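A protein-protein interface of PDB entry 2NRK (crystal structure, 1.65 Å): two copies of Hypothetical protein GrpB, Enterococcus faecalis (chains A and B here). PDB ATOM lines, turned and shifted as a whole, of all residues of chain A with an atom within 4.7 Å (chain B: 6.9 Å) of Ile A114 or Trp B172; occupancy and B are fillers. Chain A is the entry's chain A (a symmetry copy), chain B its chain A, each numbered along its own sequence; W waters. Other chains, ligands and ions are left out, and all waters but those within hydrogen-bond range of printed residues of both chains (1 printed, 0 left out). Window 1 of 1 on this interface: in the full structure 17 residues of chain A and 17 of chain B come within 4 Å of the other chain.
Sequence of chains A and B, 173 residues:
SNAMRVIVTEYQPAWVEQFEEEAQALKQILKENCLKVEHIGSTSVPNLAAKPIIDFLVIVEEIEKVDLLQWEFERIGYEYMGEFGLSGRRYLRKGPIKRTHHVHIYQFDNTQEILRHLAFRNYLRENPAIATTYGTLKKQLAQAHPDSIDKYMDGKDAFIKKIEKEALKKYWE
The indole nitrogen (NE1) of Trp B172 is in hydrogen-bond range of the backbone carbonyl oxygen (O) of Phe A108, 2.9 Å away.
The chain-end carboxylate of Glu B173 is in salt-bridge range of the side-chain amino group of Lys A36, 3.6 Å away.
O of Lys A36 sits at hydrogen-bond distance from N of Ile A59, at 2.9 Å.
OE2 of Glu B173 lies within salt-bridge range of NZ of Lys B170, 2.9 Å away.
O of Leu B168 sits close to NE1 of Trp B172, at 3.4 Å.
Lys A36 touches Trp B172 (CG to O, 3.3 Å).
Trp B172 touches Ile A59 (CD1 to CG2, 3.7 Å).
Phe A108 touches Leu B168.
CE1 of Phe A108 touches CE of Lys B169, 3.6 Å away.
CG2 of Thr A111 touches CD1 of Leu B115 (3.8 Å).
Thr A111 touches Leu B168.
CG2 of Ile A114 touches CZ3 of Trp B172, 3.4 Å away.
Leu A115 touches Leu B115 (CD1 to CD1, 3.9 Å).
Trp B172 touches Leu A115.
Leu A118 touches Trp B172.
Ile A114 touches just one residue of chain B: Trp B172 (3.4 Å).
Trp B172 touches six residues of chain A.
Of the printed residues of chain A, Leu B168 touches Phe A108 (3.7 Å) and Thr A111 (3.98 Å).
Of the printed residues of chain A, Leu B115 touches Thr A111 (3.8 Å) and Leu A115 (3.9 Å).
Printed residues of chain B within 4 Å of Leu A115: Leu B115 (3.9 Å) and Trp B172 (3.7 Å).
Of the printed residues of chain B, Thr A111 touches Leu B115 and Leu B168.
Of the printed residues of chain A, Glu B173 touches Lys A36.
Leu A57 touches none of the printed residues of chain B.
Tyr B171 touches none of the printed residues of chain A.
The nearest residue of chain B that does not touch Ile A114 is Leu B115 (6.7 Å).
Of the 8 printed residues of chain B, 5 touch a printed residue of chain A.
Printed residues of chain B that touch a printed residue of chain A: Leu B115, Leu B168, Lys B169, Trp B172 and Glu B173.
Among the printed residues, 12 pairs touch across the chains.
Among the printed residues, no Asp or Glu carboxylate lies within 4 Å of a Lys or Arg side-chain nitrogen of the other chain.
Leu A115 touches its own counterpart, Leu B115.
Position printed for both chains: 115.
Of the 12 pairs that touch across the chains among the printed residues, 1 has its exchanged pair printed and touching as well.
Water W1 lies within hydrogen-bond range of the side-chain amino group (NZ) of Lys A36 and the chain-end carboxylate (O) of Glu B173.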
ATOM      1  N   LYS A  36      17.822  -3.935 -26.920  1.00  0.00           N
ATOM      2  CA  LYS A  36      18.886  -3.859 -25.918  1.00  0.00           C
ATOM      3  C   LYS A  36      18.280  -3.538 -24.548  1.00  0.00           C
ATOM      4  O   LYS A  36      17.362  -2.745 -24.455  1.00  0.00           O
ATOM      5  CB  LYS A  36      19.876  -2.742 -26.322  1.00  0.00           C
ATOM      6  CG  LYS A  36      21.094  -2.614 -25.432  1.00  0.00           C
ATOM      7  CD  LYS A  36      22.001  -3.808 -25.647  1.00  0.00           C
ATOM      8  CE  LYS A  36      23.225  -3.665 -24.764  1.00  0.00           C
ATOM      9  NZ  LYS A  36      24.146  -4.732 -25.192  1.00  0.00           N
ATOM     10  N   LEU A  57      17.167   0.575 -18.842  1.00  0.00           N
ATOM     11  CA  LEU A  57      16.885   1.259 -20.117  1.00  0.00           C
ATOM     12  C   LEU A  57      16.612   0.169 -21.134  1.00  0.00           C
ATOM     13  O   LEU A  57      17.473  -0.659 -21.394  1.00  0.00           O
ATOM     14  CB  LEU A  57      18.077   2.121 -20.552  1.00  0.00           C
ATOM     15  CG  LEU A  57      17.935   2.802 -21.940  1.00  0.00           C
ATOM     16  CD1 LEU A  57      16.713   3.724 -22.005  1.00  0.00           C
ATOM     17  CD2 LEU A  57      19.199   3.614 -22.279  1.00  0.00           C
ATOM     18  N   ILE A  59      15.420  -0.606 -24.963  1.00  0.00           N
ATOM     19  CA  ILE A  59      15.301   0.037 -26.271  1.00  0.00           C
ATOM     20  C   ILE A  59      14.596  -0.946 -27.185  1.00  0.00           C
ATOM     21  O   ILE A  59      15.038  -2.101 -27.315  1.00  0.00           O
ATOM     22  CB  ILE A  59      16.710   0.388 -26.823  1.00  0.00           C
ATOM     23  CG1 ILE A  59      17.435   1.287 -25.818  1.00  0.00           C
ATOM     24  CG2 ILE A  59      16.555   1.026 -28.181  1.00  0.00           C
ATOM     25  CD1 ILE A  59      18.928   1.469 -26.188  1.00  0.00           C
ATOM     26  N   TYR A 106      12.050   2.900 -24.284  1.00  0.00           N
ATOM     27  CA  TYR A 106      11.923   3.885 -25.359  1.00  0.00           C
ATOM     28  C   TYR A 106      12.079   3.218 -26.728  1.00  0.00           C
ATOM     29  O   TYR A 106      12.738   2.192 -26.857  1.00  0.00           O
ATOM     30  CB  TYR A 106      13.017   4.940 -25.273  1.00  0.00           C
ATOM     31  CG  TYR A 106      13.036   5.772 -24.001  1.00  0.00           C
ATOM     32  CD1 TYR A 106      12.264   6.926 -23.880  1.00  0.00           C
ATOM     33  CD2 TYR A 106      13.904   5.429 -22.970  1.00  0.00           C
ATOM     34  CE1 TYR A 106      12.362   7.724 -22.685  1.00  0.00           C
ATOM     35  CE2 TYR A 106      13.990   6.187 -21.807  1.00  0.00           C
ATOM     36  CZ  TYR A 106      13.237   7.312 -21.676  1.00  0.00           C
ATOM     37  OH  TYR A 106      13.424   8.052 -20.500  1.00  0.00           O
ATOM     38  N   GLN A 107      11.477   3.828 -27.739  1.00  0.00           N
ATOM     39  CA  GLN A 107      11.703   3.388 -29.109  1.00  0.00           C
ATOM     40  C   GLN A 107      13.116   3.787 -29.567  1.00  0.00           C
ATOM     41  O   GLN A 107      13.656   4.811 -29.125  1.00  0.00           O
ATOM     42  CB  GLN A 107      10.681   4.028 -30.041  1.00  0.00           C
ATOM     43  CG  GLN A 107      10.543   3.301 -31.361  1.00  0.00           C
ATOM     44  CD  GLN A 107       9.244   3.686 -32.046  1.00  0.00           C
ATOM     45  OE1 GLN A 107       8.204   3.065 -31.822  1.00  0.00           O
ATOM     46  NE2 GLN A 107       9.292   4.741 -32.841  1.00  0.00           N
ATOM     47  N   PHE A 108      13.703   2.979 -30.449  1.00  0.00           N
ATOM     48  CA  PHE A 108      15.072   3.177 -30.917  1.00  0.00           C
ATOM     49  C   PHE A 108      15.395   4.601 -31.472  1.00  0.00           C
ATOM     50  O   PHE A 108      16.568   4.996 -31.548  1.00  0.00           O
ATOM     51  CB  PHE A 108      15.380   2.185 -32.053  1.00  0.00           C
ATOM     52  CG  PHE A 108      14.700   2.540 -33.330  1.00  0.00           C
ATOM     53  CD1 PHE A 108      13.363   2.195 -33.524  1.00  0.00           C
ATOM     54  CD2 PHE A 108      15.374   3.253 -34.326  1.00  0.00           C
ATOM     55  CE1 PHE A 108      12.701   2.532 -34.693  1.00  0.00           C
ATOM     56  CE2 PHE A 108      14.724   3.611 -35.508  1.00  0.00           C
ATOM     57  CZ  PHE A 108      13.385   3.254 -35.699  1.00  0.00           C
ATOM     58  N   ASN A 110      14.200   7.471 -30.269  1.00  0.00           N
ATOM     59  CA  ASN A 110      14.214   8.504 -29.244  1.00  0.00           C
ATOM     60  C   ASN A 110      15.629   8.717 -28.748  1.00  0.00           C
ATOM     61  O   ASN A 110      15.976   8.401 -27.603  1.00  0.00           O
ATOM     62  CB  ASN A 110      13.273   8.116 -28.109  1.00  0.00           C
ATOM     63  CG  ASN A 110      12.912   9.317 -27.234  1.00  0.00           C
ATOM     64  OD1 ASN A 110      13.695  10.289 -27.106  1.00  0.00           O
ATOM     65  ND2 ASN A 110      11.749   9.241 -26.601  1.00  0.00           N
ATOM     66  N   THR A 111      16.470   9.234 -29.637  1.00  0.00           N
ATOM     67  CA  THR A 111      17.908   9.355 -29.325  1.00  0.00           C
ATOM     68  C   THR A 111      18.176  10.293 -28.159  1.00  0.00           C
ATOM     69  O   THR A 111      19.130  10.082 -27.410  1.00  0.00           O
ATOM     70  CB  THR A 111      18.716   9.782 -30.535  1.00  0.00           C
ATOM     71  OG1 THR A 111      18.326  11.108 -30.952  1.00  0.00           O
ATOM     72  CG2 THR A 111      18.480   8.778 -31.698  1.00  0.00           C
ATOM     73  N   GLN A 112      17.361  11.344 -28.000  1.00  0.00           N
ATOM     74  CA  GLN A 112      17.610  12.309 -26.917  1.00  0.00           C
ATOM     75  C   GLN A 112      17.532  11.637 -25.548  1.00  0.00           C
ATOM     76  O   GLN A 112      18.408  11.846 -24.705  1.00  0.00           O
ATOM     77  CB  GLN A 112      16.619  13.482 -26.978  1.00  0.00           C
ATOM     78  CG  GLN A 112      16.621  14.252 -28.292  1.00  0.00           C
ATOM     79  CD  GLN A 112      17.678  15.324 -28.351  1.00  0.00           C
ATOM     80  OE1 GLN A 112      18.866  15.033 -28.372  1.00  0.00           O
ATOM     81  NE2 GLN A 112      17.246  16.583 -28.398  1.00  0.00           N
ATOM     82  N   GLU A 113      16.485  10.835 -25.331  1.00  0.00           N
ATOM     83  CA  GLU A 113      16.302  10.196 -24.008  1.00  0.00           C
ATOM     84  C   GLU A 113      17.277   9.070 -23.836  1.00  0.00           C
ATOM     85  O   GLU A 113      17.852   8.892 -22.761  1.00  0.00           O
ATOM     86  CB  GLU A 113      14.878   9.692 -23.880  1.00  0.00           C
ATOM     87  CG  GLU A 113      13.951  10.857 -23.527  1.00  0.00           C
ATOM     88  CD  GLU A 113      14.277  11.359 -22.106  1.00  0.00           C
ATOM     89  OE1 GLU A 113      14.072  10.591 -21.126  1.00  0.00           O
ATOM     90  OE2 GLU A 113      14.748  12.489 -21.978  1.00  0.00           O
ATOM     91  N   ILE A 114      17.468   8.293 -24.909  1.00  0.00           N
ATOM     92  CA  ILE A 114      18.394   7.157 -24.775  1.00  0.00           C
ATOM     93  C   ILE A 114      19.798   7.633 -24.430  1.00  0.00           C
ATOM     94  O   ILE A 114      20.426   7.140 -23.490  1.00  0.00           O
ATOM     95  CB  ILE A 114      18.390   6.274 -26.053  1.00  0.00           C
ATOM     96  CG1 ILE A 114      16.984   5.652 -26.241  1.00  0.00           C
ATOM     97  CG2 ILE A 114      19.501   5.195 -25.964  1.00  0.00           C
ATOM     98  CD1 ILE A 114      16.740   5.050 -27.661  1.00  0.00           C
ATOM     99  N   LEU A 115      20.299   8.605 -25.194  1.00  0.00           N
ATOM    100  CA  LEU A 115      21.640   9.168 -24.876  1.00  0.00           C
ATOM    101  C   LEU A 115      21.703   9.925 -23.572  1.00  0.00           C
ATOM    102  O   LEU A 115      22.743   9.906 -22.919  1.00  0.00           O
ATOM    103  CB  LEU A 115      22.217  10.018 -26.023  1.00  0.00           C
ATOM    104  CG  LEU A 115      22.605   9.203 -27.256  1.00  0.00           C
ATOM    105  CD1 LEU A 115      23.354  10.122 -28.214  1.00  0.00           C
ATOM    106  CD2 LEU A 115      23.528   7.979 -26.944  1.00  0.00           C
ATOM    107  N   ARG A 116      20.606  10.564 -23.155  1.00  0.00           N
ATOM    108  CA  ARG A 116      20.621  11.282 -21.869  1.00  0.00           C
ATOM    109  C   ARG A 116      21.056  10.295 -20.787  1.00  0.00           C
ATOM    110  O   ARG A 116      21.953  10.582 -19.993  1.00  0.00           O
ATOM    111  CB  ARG A 116      19.252  11.835 -21.525  1.00  0.00           C
ATOM    112  CG  ARG A 116      19.289  12.523 -20.129  1.00  0.00           C
ATOM    113  CD  ARG A 116      18.025  13.380 -19.955  1.00  0.00           C
ATOM    114  NE  ARG A 116      16.822  12.565 -19.831  1.00  0.00           N
ATOM    115  CZ  ARG A 116      16.380  12.042 -18.691  1.00  0.00           C
ATOM    116  NH1 ARG A 116      17.092  12.184 -17.551  1.00  0.00           N
ATOM    117  NH2 ARG A 116      15.242  11.338 -18.697  1.00  0.00           N
ATOM    118  N   HIS A 117      20.427   9.109 -20.790  1.00  0.00           N
ATOM    119  CA  HIS A 117      20.736   8.100 -19.782  1.00  0.00           C
ATOM    120  C   HIS A 117      22.108   7.484 -19.984  1.00  0.00           C
ATOM    121  O   HIS A 117      22.863   7.379 -19.027  1.00  0.00           O
ATOM    122  CB  HIS A 117      19.684   6.981 -19.808  1.00  0.00           C
ATOM    123  CG  HIS A 117      18.317   7.440 -19.409  1.00  0.00           C
ATOM    124  ND1 HIS A 117      18.047   7.946 -18.152  1.00  0.00           N
ATOM    125  CD2 HIS A 117      17.142   7.463 -20.087  1.00  0.00           C
ATOM    126  CE1 HIS A 117      16.757   8.242 -18.067  1.00  0.00           C
ATOM    127  NE2 HIS A 117      16.189   7.981 -19.234  1.00  0.00           N
ATOM    128  N   LEU A 118      22.433   7.059 -21.211  1.00  0.00           N
ATOM    129  CA  LEU A 118      23.696   6.344 -21.407  1.00  0.00           C
ATOM    130  C   LEU A 118      24.889   7.280 -21.221  1.00  0.00           C
ATOM    131  O   LEU A 118      25.888   6.886 -20.628  1.00  0.00           O
ATOM    132  CB  LEU A 118      23.776   5.684 -22.804  1.00  0.00           C
ATOM    133  CG  LEU A 118      22.763   4.553 -22.991  1.00  0.00           C
ATOM    134  CD1 LEU A 118      22.782   4.122 -24.491  1.00  0.00           C
ATOM    135  CD2 LEU A 118      23.085   3.365 -22.062  1.00  0.00           C
ATOM    136  N   LEU B 115      23.382  11.129 -34.612  1.00  0.00           N
ATOM    137  CA  LEU B 115      23.233   9.657 -34.783  1.00  0.00           C
ATOM    138  C   LEU B 115      22.727   9.238 -36.142  1.00  0.00           C
ATOM    139  O   LEU B 115      23.109   8.173 -36.619  1.00  0.00           O
ATOM    140  CB  LEU B 115      22.391   9.010 -33.669  1.00  0.00           C
ATOM    141  CG  LEU B 115      23.077   9.006 -32.304  1.00  0.00           C
ATOM    142  CD1 LEU B 115      22.240   8.154 -31.356  1.00  0.00           C
ATOM    143  CD2 LEU B 115      24.527   8.421 -32.323  1.00  0.00           C
ATOM    144  N   ALA B 167      19.787   1.188 -39.568  1.00  0.00           N
ATOM    145  CA  ALA B 167      21.073   1.528 -38.968  1.00  0.00           C
ATOM    146  C   ALA B 167      20.915   1.983 -37.514  1.00  0.00           C
ATOM    147  O   ALA B 167      21.707   1.596 -36.650  1.00  0.00           O
ATOM    148  CB  ALA B 167      21.731   2.645 -39.770  1.00  0.00           C
ATOM    149  N   LEU B 168      19.891   2.804 -37.262  1.00  0.00           N
ATOM    150  CA  LEU B 168      19.695   3.365 -35.912  1.00  0.00           C
ATOM    151  C   LEU B 168      19.256   2.247 -34.950  1.00  0.00           C
ATOM    152  O   LEU B 168      19.680   2.237 -33.790  1.00  0.00           O
ATOM    153  CB  LEU B 168      18.686   4.509 -35.931  1.00  0.00           C
ATOM    154  CG  LEU B 168      18.606   5.354 -34.641  1.00  0.00           C
ATOM    155  CD1 LEU B 168      20.027   5.874 -34.225  1.00  0.00           C
ATOM    156  CD2 LEU B 168      17.587   6.489 -34.828  1.00  0.00           C
ATOM    157  N   LYS B 169      18.431   1.315 -35.430  1.00  0.00           N
ATOM    158  CA  LYS B 169      18.074   0.137 -34.622  1.00  0.00           C
ATOM    159  C   LYS B 169      19.349  -0.623 -34.239  1.00  0.00           C
ATOM    160  O   LYS B 169      19.544  -0.982 -33.079  1.00  0.00           O
ATOM    161  CB  LYS B 169      17.103  -0.787 -35.371  1.00  0.00           C
ATOM    162  CG  LYS B 169      15.719  -0.170 -35.526  1.00  0.00           C
ATOM    163  CD  LYS B 169      14.815  -1.047 -36.400  1.00  0.00           C
ATOM    164  CE  LYS B 169      13.411  -0.456 -36.511  1.00  0.00           C
ATOM    165  NZ  LYS B 169      12.579  -1.378 -37.343  1.00  0.00           N
ATOM    166  N   LYS B 170      20.218  -0.847 -35.224  1.00  0.00           N
ATOM    167  CA  LYS B 170      21.440  -1.635 -35.009  1.00  0.00           C
ATOM    168  C   LYS B 170      22.413  -0.940 -34.055  1.00  0.00           C
ATOM    169  O   LYS B 170      23.162  -1.615 -33.300  1.00  0.00           O
ATOM    170  CB  LYS B 170      22.130  -1.921 -36.370  1.00  0.00           C
ATOM    171  CG  LYS B 170      23.352  -2.867 -36.266  1.00  0.00           C
ATOM    172  CD  LYS B 170      22.994  -4.304 -35.765  1.00  0.00           C
ATOM    173  CE  LYS B 170      21.938  -5.011 -36.612  1.00  0.00           C
ATOM    174  NZ  LYS B 170      21.486  -6.381 -36.096  1.00  0.00           N
ATOM    175  N   TYR B 171      22.406   0.387 -34.096  1.00  0.00           N
ATOM    176  CA  TYR B 171      23.322   1.228 -33.306  1.00  0.00           C
ATOM    177  C   TYR B 171      23.286   0.828 -31.813  1.00  0.00           C
ATOM    178  O   TYR B 171      24.303   0.873 -31.135  1.00  0.00           O
ATOM    179  CB  TYR B 171      22.960   2.718 -33.456  1.00  0.00           C
ATOM    180  CG  TYR B 171      23.949   3.630 -32.767  1.00  0.00           C
ATOM    181  CD1 TYR B 171      25.174   3.978 -33.385  1.00  0.00           C
ATOM    182  CD2 TYR B 171      23.694   4.123 -31.477  1.00  0.00           C
ATOM    183  CE1 TYR B 171      26.090   4.819 -32.705  1.00  0.00           C
ATOM    184  CE2 TYR B 171      24.604   4.966 -30.810  1.00  0.00           C
ATOM    185  CZ  TYR B 171      25.801   5.304 -31.413  1.00  0.00           C
ATOM    186  OH  TYR B 171      26.672   6.113 -30.695  1.00  0.00           O
ATOM    187  N   TRP B 172      22.094   0.457 -31.304  1.00  0.00           N
ATOM    188  CA  TRP B 172      21.904   0.189 -29.858  1.00  0.00           C
ATOM    189  C   TRP B 172      22.236  -1.243 -29.459  1.00  0.00           C
ATOM    190  O   TRP B 172      22.350  -1.545 -28.275  1.00  0.00           O
ATOM    191  CB  TRP B 172      20.439   0.470 -29.453  1.00  0.00           C
ATOM    192  CG  TRP B 172      20.024   1.825 -29.784  1.00  0.00           C
ATOM    193  CD1 TRP B 172      19.012   2.190 -30.629  1.00  0.00           C
ATOM    194  CD2 TRP B 172      20.625   3.049 -29.321  1.00  0.00           C
ATOM    195  NE1 TRP B 172      18.924   3.543 -30.695  1.00  0.00           N
ATOM    196  CE2 TRP B 172      19.910   4.112 -29.918  1.00  0.00           C
ATOM    197  CE3 TRP B 172      21.702   3.350 -28.460  1.00  0.00           C
ATOM    198  CZ2 TRP B 172      20.232   5.461 -29.701  1.00  0.00           C
ATOM    199  CZ3 TRP B 172      22.025   4.710 -28.235  1.00  0.00           C
ATOM    200  CH2 TRP B 172      21.292   5.746 -28.841  1.00  0.00           C
ATOM    201  N   GLU B 173      22.370  -2.132 -30.449  1.00  0.00           N
ATOM    202  CA  GLU B 173      22.455  -3.559 -30.143  1.00  0.00           C
ATOM    203  C   GLU B 173      23.788  -3.936 -29.532  1.00  0.00           C
ATOM    204  O   GLU B 173      23.871  -4.926 -28.784  1.00  0.00           O
ATOM    205  CB  GLU B 173      22.168  -4.412 -31.384  1.00  0.00           C
ATOM    206  CG  GLU B 173      20.700  -4.364 -31.799  1.00  0.00           C
ATOM    207  CD  GLU B 173      20.351  -5.428 -32.835  1.00  0.00           C
ATOM    208  OE1 GLU B 173      20.362  -6.621 -32.486  1.00  0.00           O
ATOM    209  OE2 GLU B 173      20.047  -5.070 -33.990  1.00  0.00           O
ATOM    210  OXT GLU B 173      24.782  -3.249 -29.753  1.00  0.00           O
HETATM  211  O   HOH W   1      25.696  -4.546 -27.099  1.00  0.00           O
